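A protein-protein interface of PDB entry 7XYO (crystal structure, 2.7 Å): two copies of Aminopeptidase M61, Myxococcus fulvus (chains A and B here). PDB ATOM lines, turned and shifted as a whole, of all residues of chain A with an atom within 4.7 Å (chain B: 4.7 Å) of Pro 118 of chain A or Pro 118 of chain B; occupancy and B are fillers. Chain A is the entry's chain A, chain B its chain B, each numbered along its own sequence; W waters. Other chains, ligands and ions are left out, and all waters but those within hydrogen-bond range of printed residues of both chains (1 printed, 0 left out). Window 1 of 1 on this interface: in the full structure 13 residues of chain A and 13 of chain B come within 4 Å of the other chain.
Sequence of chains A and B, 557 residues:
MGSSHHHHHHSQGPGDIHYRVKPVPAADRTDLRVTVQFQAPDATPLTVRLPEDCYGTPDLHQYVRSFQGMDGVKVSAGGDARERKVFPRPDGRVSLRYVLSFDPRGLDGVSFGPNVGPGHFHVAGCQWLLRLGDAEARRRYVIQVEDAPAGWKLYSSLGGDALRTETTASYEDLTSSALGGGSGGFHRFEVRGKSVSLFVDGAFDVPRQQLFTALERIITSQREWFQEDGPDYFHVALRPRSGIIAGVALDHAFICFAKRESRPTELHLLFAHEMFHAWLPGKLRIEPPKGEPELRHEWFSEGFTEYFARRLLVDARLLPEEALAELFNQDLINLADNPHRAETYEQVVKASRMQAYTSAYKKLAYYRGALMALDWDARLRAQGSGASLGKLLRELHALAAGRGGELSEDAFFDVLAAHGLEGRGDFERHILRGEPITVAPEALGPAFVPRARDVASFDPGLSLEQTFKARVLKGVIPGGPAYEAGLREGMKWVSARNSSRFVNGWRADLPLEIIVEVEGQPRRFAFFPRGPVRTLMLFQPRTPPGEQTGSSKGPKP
Of the 12 printed residues of chain B, 2 touch a printed residue of chain A.
Hydrophobic or aromatic side chains of chain B within 4 Å of the printed part of chain A: Pro 118 and Ala 203.
Printed residues of chain A that touch a printed residue of chain B: Pro 118 and Ala 203.
Hydrophobic or aromatic side chains of chain A that line the printed part of chain B: Pro 118 and Ala 203.
Among the printed residues, no Asp or Glu carboxylate lies within 4 Å of a Lys or Arg side-chain nitrogen of the other chain.
Water W1 lies within hydrogen-bond range of the side-chain carboxylate of Asp 28 of chain A (2.4 Å) and the side-chain carboxylate of Asp 28 of chain B (2.6 Å).
Among the printed residues, merely in contact across the chains: Ala 203 of chain A with Pro 118 of chain B (3.7 Å), Pro 118 of chain A with Pro 118 of chain B (3.8 Å) and Pro 118 of chain A with Ala 203 of chain B (3.9 Å).
Pro 118 of chain A touches its own counterpart, Pro 118 of chain B.
Pro 118 of chain A touches Ala 203 of chain B, and with the chains exchanged Ala 203 of chain A touches Pro 118 of chain B.
Of the 3 pairs that touch across the chains among the printed residues, 3 have their exchanged pair printed and touching as well.
Arg 29 of chain A touches none of the printed residues of chain B.
Printed residues of chain B within 4 Å of Ala 203 of chain A: Pro 118.
Thr 30 of chain B touches none of the printed residues of chain A.
Pro 118 of chain B touches two residues of chain A.
Printed residues of chain A within 4 Å of Ala 203 of chain B: Pro 118 (3.9 Å).
The nearest printed residue of chain A that does not touch Pro 118 of chain B is Asp 28 of chain A (6.0 Å).
The nearest printed residue of chain A that does not touch Ala 203 of chain B is Gly 119 of chain A (5.0 Å).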
ATOM      1  N   PRO A  25       9.567  10.457 -30.121  1.00  0.00           N
ATOM      2  CA  PRO A  25      10.030   9.249 -29.428  1.00  0.00           C
ATOM      3  C   PRO A  25      10.583   8.226 -30.407  1.00  0.00           C
ATOM      4  O   PRO A  25      10.143   8.124 -31.554  1.00  0.00           O
ATOM      5  CB  PRO A  25       8.768   8.727 -28.731  1.00  0.00           C
ATOM      6  CG  PRO A  25       7.846   9.889 -28.658  1.00  0.00           C
ATOM      7  CD  PRO A  25       8.158  10.768 -29.828  1.00  0.00           C
ATOM      8  N   ALA A  26      11.565   7.462 -29.936  1.00  0.00           N
ATOM      9  CA  ALA A  26      12.220   6.446 -30.747  1.00  0.00           C
ATOM     10  C   ALA A  26      12.403   5.197 -29.891  1.00  0.00           C
ATOM     11  O   ALA A  26      11.869   5.094 -28.782  1.00  0.00           O
ATOM     12  CB  ALA A  26      13.549   6.968 -31.308  1.00  0.00           C
ATOM     13  N   ALA A  27      13.174   4.243 -30.416  1.00  0.00           N
ATOM     14  CA  ALA A  27      13.347   2.963 -29.735  1.00  0.00           C
ATOM     15  C   ALA A  27      14.098   3.130 -28.419  1.00  0.00           C
ATOM     16  O   ALA A  27      13.649   2.652 -27.372  1.00  0.00           O
ATOM     17  CB  ALA A  27      14.075   1.979 -30.650  1.00  0.00           C
ATOM     18  N   ASP A  28      15.247   3.805 -28.454  1.00  0.00           N
ATOM     19  CA  ASP A  28      16.095   3.952 -27.280  1.00  0.00           C
ATOM     20  C   ASP A  28      16.225   5.391 -26.803  1.00  0.00           C
ATOM     21  O   ASP A  28      16.873   5.629 -25.778  1.00  0.00           O
ATOM     22  CB  ASP A  28      17.490   3.380 -27.562  1.00  0.00           C
ATOM     23  CG  ASP A  28      18.276   4.212 -28.563  1.00  0.00           C
ATOM     24  OD1 ASP A  28      17.654   4.941 -29.365  1.00  0.00           O
ATOM     25  OD2 ASP A  28      19.524   4.132 -28.549  1.00  0.00           O
ATOM     26  N   ARG A  29      15.632   6.351 -27.503  1.00  0.00           N
ATOM     27  CA  ARG A  29      15.842   7.756 -27.190  1.00  0.00           C
ATOM     28  C   ARG A  29      14.605   8.545 -27.607  1.00  0.00           C
ATOM     29  O   ARG A  29      13.594   7.976 -28.028  1.00  0.00           O
ATOM     30  CB  ARG A  29      17.101   8.274 -27.895  1.00  0.00           C
ATOM     31  CG  ARG A  29      16.957   8.322 -29.406  1.00  0.00           C
ATOM     32  CD  ARG A  29      18.293   8.504 -30.095  1.00  0.00           C
ATOM     33  NE  ARG A  29      19.139   7.324 -29.982  1.00  0.00           N
ATOM     34  CZ  ARG A  29      20.388   7.257 -30.422  1.00  0.00           C
ATOM     35  NH1 ARG A  29      20.966   8.287 -31.018  1.00  0.00           N
ATOM     36  NH2 ARG A  29      21.073   6.128 -30.263  1.00  0.00           N
ATOM     37  N   THR A  30      14.694   9.868 -27.480  1.00  0.00           N
ATOM     38  CA  THR A  30      13.683  10.791 -27.985  1.00  0.00           C
ATOM     39  C   THR A  30      14.408  11.876 -28.768  1.00  0.00           C
ATOM     40  O   THR A  30      15.150  12.675 -28.187  1.00  0.00           O
ATOM     41  CB  THR A  30      12.856  11.396 -26.851  1.00  0.00           C
ATOM     42  OG1 THR A  30      12.022  10.386 -26.272  1.00  0.00           O
ATOM     43  CG2 THR A  30      11.984  12.529 -27.373  1.00  0.00           C
ATOM     44  N   GLY A 117      15.836   9.542 -23.640  1.00  0.00           N
ATOM     45  CA  GLY A 117      15.547   8.151 -23.629  1.00  0.00           C
ATOM     46  C   GLY A 117      14.160   7.863 -24.110  1.00  0.00           C
ATOM     47  O   GLY A 117      13.469   8.751 -24.417  1.00  0.00           O
ATOM     48  N   PRO A 118      13.714   6.614 -24.142  1.00  0.00           N
ATOM     49  CA  PRO A 118      12.442   6.291 -24.791  1.00  0.00           C
ATOM     50  C   PRO A 118      11.145   7.028 -24.463  1.00  0.00           C
ATOM     51  O   PRO A 118      10.265   7.072 -25.278  1.00  0.00           O
ATOM     52  CB  PRO A 118      12.307   4.817 -24.519  1.00  0.00           C
ATOM     53  CG  PRO A 118      13.143   4.569 -23.397  1.00  0.00           C
ATOM     54  CD  PRO A 118      14.311   5.385 -23.641  1.00  0.00           C
ATOM     55  N   GLY A 119      11.051   7.589 -23.293  1.00  0.00           N
ATOM     56  CA  GLY A 119       9.901   8.294 -22.904  1.00  0.00           C
ATOM     57  C   GLY A 119      10.116   9.665 -22.330  1.00  0.00           C
ATOM     58  O   GLY A 119       9.255  10.131 -21.673  1.00  0.00           O
ATOM     59  N   HIS A 120      11.217  10.351 -22.540  1.00  0.00           N
ATOM     60  CA  HIS A 120      11.532  11.639 -21.931  1.00  0.00           C
ATOM     61  C   HIS A 120      12.670  12.293 -22.698  1.00  0.00           C
ATOM     62  O   HIS A 120      13.304  11.679 -23.560  1.00  0.00           O
ATOM     63  CB  HIS A 120      11.910  11.485 -20.456  1.00  0.00           C
ATOM     64  CG  HIS A 120      13.346  11.121 -20.237  1.00  0.00           C
ATOM     65  ND1 HIS A 120      13.806   9.824 -20.309  1.00  0.00           N
ATOM     66  CD2 HIS A 120      14.425  11.887 -19.947  1.00  0.00           C
ATOM     67  CE1 HIS A 120      15.105   9.805 -20.073  1.00  0.00           C
ATOM     68  NE2 HIS A 120      15.506  11.044 -19.851  1.00  0.00           N
ATOM     69  N   TRP A 152       2.279  13.304 -22.461  1.00  0.00           N
ATOM     70  CA  TRP A 152       3.553  13.818 -21.987  1.00  0.00           C
ATOM     71  C   TRP A 152       3.358  15.163 -21.300  1.00  0.00           C
ATOM     72  O   TRP A 152       2.494  15.959 -21.679  1.00  0.00           O
ATOM     73  CB  TRP A 152       4.548  13.966 -23.140  1.00  0.00           C
ATOM     74  CG  TRP A 152       5.152  12.670 -23.593  1.00  0.00           C
ATOM     75  CD1 TRP A 152       4.529  11.459 -23.682  1.00  0.00           C
ATOM     76  CD2 TRP A 152       6.504  12.458 -24.020  1.00  0.00           C
ATOM     77  NE1 TRP A 152       5.409  10.506 -24.139  1.00  0.00           N
ATOM     78  CE2 TRP A 152       6.628  11.094 -24.353  1.00  0.00           C
ATOM     79  CE3 TRP A 152       7.621  13.290 -24.152  1.00  0.00           C
ATOM     80  CZ2 TRP A 152       7.823  10.543 -24.811  1.00  0.00           C
ATOM     81  CZ3 TRP A 152       8.807  12.741 -24.606  1.00  0.00           C
ATOM     82  CH2 TRP A 152       8.898  11.381 -24.930  1.00  0.00           C
ATOM     83  N   ALA A 203      14.945   4.777 -14.547  1.00  0.00           N
ATOM     84  CA  ALA A 203      14.810   3.736 -13.539  1.00  0.00           C
ATOM     85  C   ALA A 203      15.309   4.240 -12.192  1.00  0.00           C
ATOM     86  O   ALA A 203      16.420   4.770 -12.089  1.00  0.00           O
ATOM     87  CB  ALA A 203      15.579   2.484 -13.958  1.00  0.00           C
ATOM     88  N   PRO B  25      19.782  -3.421 -15.090  1.00  0.00           N
ATOM     89  CA  PRO B  25      19.389  -2.258 -15.848  1.00  0.00           C
ATOM     90  C   PRO B  25      20.572  -1.448 -16.267  1.00  0.00           C
ATOM     91  O   PRO B  25      21.476  -1.275 -15.528  1.00  0.00           O
ATOM     92  CB  PRO B  25      18.511  -1.514 -14.874  1.00  0.00           C
ATOM     93  CG  PRO B  25      18.032  -2.523 -13.948  1.00  0.00           C
ATOM     94  CD  PRO B  25      19.174  -3.418 -13.763  1.00  0.00           C
ATOM     95  N   ALA B  26      20.535  -0.966 -17.488  1.00  0.00           N
ATOM     96  CA  ALA B  26      21.595  -0.179 -18.094  1.00  0.00           C
ATOM     97  C   ALA B  26      21.016   1.145 -18.587  1.00  0.00           C
ATOM     98  O   ALA B  26      19.861   1.481 -18.318  1.00  0.00           O
ATOM     99  CB  ALA B  26      22.265  -0.965 -19.222  1.00  0.00           C
ATOM    100  N   ALA B  27      21.835   1.895 -19.325  1.00  0.00           N
ATOM    101  CA  ALA B  27      21.425   3.220 -19.775  1.00  0.00           C
ATOM    102  C   ALA B  27      20.301   3.140 -20.799  1.00  0.00           C
ATOM    103  O   ALA B  27      19.321   3.889 -20.712  1.00  0.00           O
ATOM    104  CB  ALA B  27      22.623   3.970 -20.356  1.00  0.00           C
ATOM    105  N   ASP B  28      20.421   2.242 -21.776  1.00  0.00           N
ATOM    106  CA  ASP B  28      19.441   2.125 -22.845  1.00  0.00           C
ATOM    107  C   ASP B  28      18.775   0.759 -22.912  1.00  0.00           C
ATOM    108  O   ASP B  28      17.971   0.524 -23.822  1.00  0.00           O
ATOM    109  CB  ASP B  28      20.094   2.434 -24.201  1.00  0.00           C
ATOM    110  CG  ASP B  28      21.003   1.316 -24.682  1.00  0.00           C
ATOM    111  OD1 ASP B  28      21.587   0.606 -23.835  1.00  0.00           O
ATOM    112  OD2 ASP B  28      21.134   1.147 -25.913  1.00  0.00           O
ATOM    113  N   ARG B  29      19.077  -0.144 -21.984  1.00  0.00           N
ATOM    114  CA  ARG B  29      18.586  -1.513 -22.066  1.00  0.00           C
ATOM    115  C   ARG B  29      18.651  -2.142 -20.681  1.00  0.00           C
ATOM    116  O   ARG B  29      19.018  -1.494 -19.697  1.00  0.00           O
ATOM    117  CB  ARG B  29      19.401  -2.324 -23.074  1.00  0.00           C
ATOM    118  CG  ARG B  29      20.825  -2.591 -22.614  1.00  0.00           C
ATOM    119  CD  ARG B  29      21.712  -3.036 -23.759  1.00  0.00           C
ATOM    120  NE  ARG B  29      21.840  -2.007 -24.784  1.00  0.00           N
ATOM    121  CZ  ARG B  29      22.604  -2.118 -25.862  1.00  0.00           C
ATOM    122  NH1 ARG B  29      23.331  -3.200 -26.084  1.00  0.00           N
ATOM    123  NH2 ARG B  29      22.640  -1.117 -26.737  1.00  0.00           N
ATOM    124  N   THR B  30      18.289  -3.422 -20.616  1.00  0.00           N
ATOM    125  CA  THR B  30      18.459  -4.238 -19.418  1.00  0.00           C
ATOM    126  C   THR B  30      19.181  -5.513 -19.829  1.00  0.00           C
ATOM    127  O   THR B  30      18.625  -6.337 -20.563  1.00  0.00           O
ATOM    128  CB  THR B  30      17.117  -4.559 -18.759  1.00  0.00           C
ATOM    129  OG1 THR B  30      16.576  -3.371 -18.169  1.00  0.00           O
ATOM    130  CG2 THR B  30      17.294  -5.623 -17.681  1.00  0.00           C
ATOM    131  N   GLY B 117      14.591  -2.692 -22.469  1.00  0.00           N
ATOM    132  CA  GLY B 117      14.527  -1.268 -22.250  1.00  0.00           C
ATOM    133  C   GLY B 117      15.159  -0.899 -20.925  1.00  0.00           C
ATOM    134  O   GLY B 117      15.470  -1.765 -20.101  1.00  0.00           O
ATOM    135  N   PRO B 118      15.364   0.401 -20.691  1.00  0.00           N
ATOM    136  CA  PRO B 118      15.995   0.834 -19.432  1.00  0.00           C
ATOM    137  C   PRO B 118      15.234   0.420 -18.179  1.00  0.00           C
ATOM    138  O   PRO B 118      15.788   0.545 -17.079  1.00  0.00           O
ATOM    139  CB  PRO B 118      16.052   2.365 -19.562  1.00  0.00           C
ATOM    140  CG  PRO B 118      15.240   2.713 -20.773  1.00  0.00           C
ATOM    141  CD  PRO B 118      15.192   1.508 -21.644  1.00  0.00           C
ATOM    142  N   GLY B 119      14.002  -0.071 -18.302  1.00  0.00           N
ATOM    143  CA  GLY B 119      13.248  -0.487 -17.137  1.00  0.00           C
ATOM    144  C   GLY B 119      12.398  -1.726 -17.345  1.00  0.00           C
ATOM    145  O   GLY B 119      11.405  -1.919 -16.639  1.00  0.00           O
ATOM    146  N   HIS B 120      12.776  -2.574 -18.301  1.00  0.00           N
ATOM    147  CA  HIS B 120      12.021  -3.787 -18.585  1.00  0.00           C
ATOM    148  C   HIS B 120      12.875  -4.728 -19.423  1.00  0.00           C
ATOM    149  O   HIS B 120      13.935  -4.355 -19.932  1.00  0.00           O
ATOM    150  CB  HIS B 120      10.707  -3.476 -19.308  1.00  0.00           C
ATOM    151  CG  HIS B 120      10.851  -3.331 -20.792  1.00  0.00           C
ATOM    152  ND1 HIS B 120      11.179  -2.135 -21.395  1.00  0.00           N
ATOM    153  CD2 HIS B 120      10.706  -4.229 -21.795  1.00  0.00           C
ATOM    154  CE1 HIS B 120      11.233  -2.304 -22.704  1.00  0.00           C
ATOM    155  NE2 HIS B 120      10.950  -3.566 -22.973  1.00  0.00           N
ATOM    156  N   TRP B 152      10.352  -3.895  -9.292  1.00  0.00           N
ATOM    157  CA  TRP B 152      10.016  -4.545 -10.512  1.00  0.00           C
ATOM    158  C   TRP B 152       9.148  -5.716 -10.303  1.00  0.00           C
ATOM    159  O   TRP B 152       9.236  -6.376  -9.328  1.00  0.00           O
ATOM    160  CB  TRP B 152      11.256  -5.047 -11.172  1.00  0.00           C
ATOM    161  CG  TRP B 152      12.016  -4.036 -11.812  1.00  0.00           C
ATOM    162  CD1 TRP B 152      12.091  -2.773 -11.464  1.00  0.00           C
ATOM    163  CD2 TRP B 152      12.769  -4.168 -13.000  1.00  0.00           C
ATOM    164  NE1 TRP B 152      12.905  -2.107 -12.288  1.00  0.00           N
ATOM    165  CE2 TRP B 152      13.311  -2.949 -13.261  1.00  0.00           C
ATOM    166  CE3 TRP B 152      13.014  -5.201 -13.881  1.00  0.00           C
ATOM    167  CZ2 TRP B 152      14.096  -2.724 -14.298  1.00  0.00           C
ATOM    168  CZ3 TRP B 152      13.795  -4.959 -14.931  1.00  0.00           C
ATOM    169  CH2 TRP B 152      14.342  -3.741 -15.137  1.00  0.00           C
ATOM    170  N   ALA B 203       6.791   3.155 -24.419  1.00  0.00           N
ATOM    171  CA  ALA B 203       5.985   4.335 -24.618  1.00  0.00           C
ATOM    172  C   ALA B 203       4.693   4.018 -25.309  1.00  0.00           C
ATOM    173  O   ALA B 203       4.722   3.386 -26.277  1.00  0.00           O
ATOM    174  CB  ALA B 203       6.742   5.322 -25.435  1.00  0.00           C
HETATM  175  O   HOH W   1      21.267   2.467 -28.190  1.00  0.00           O
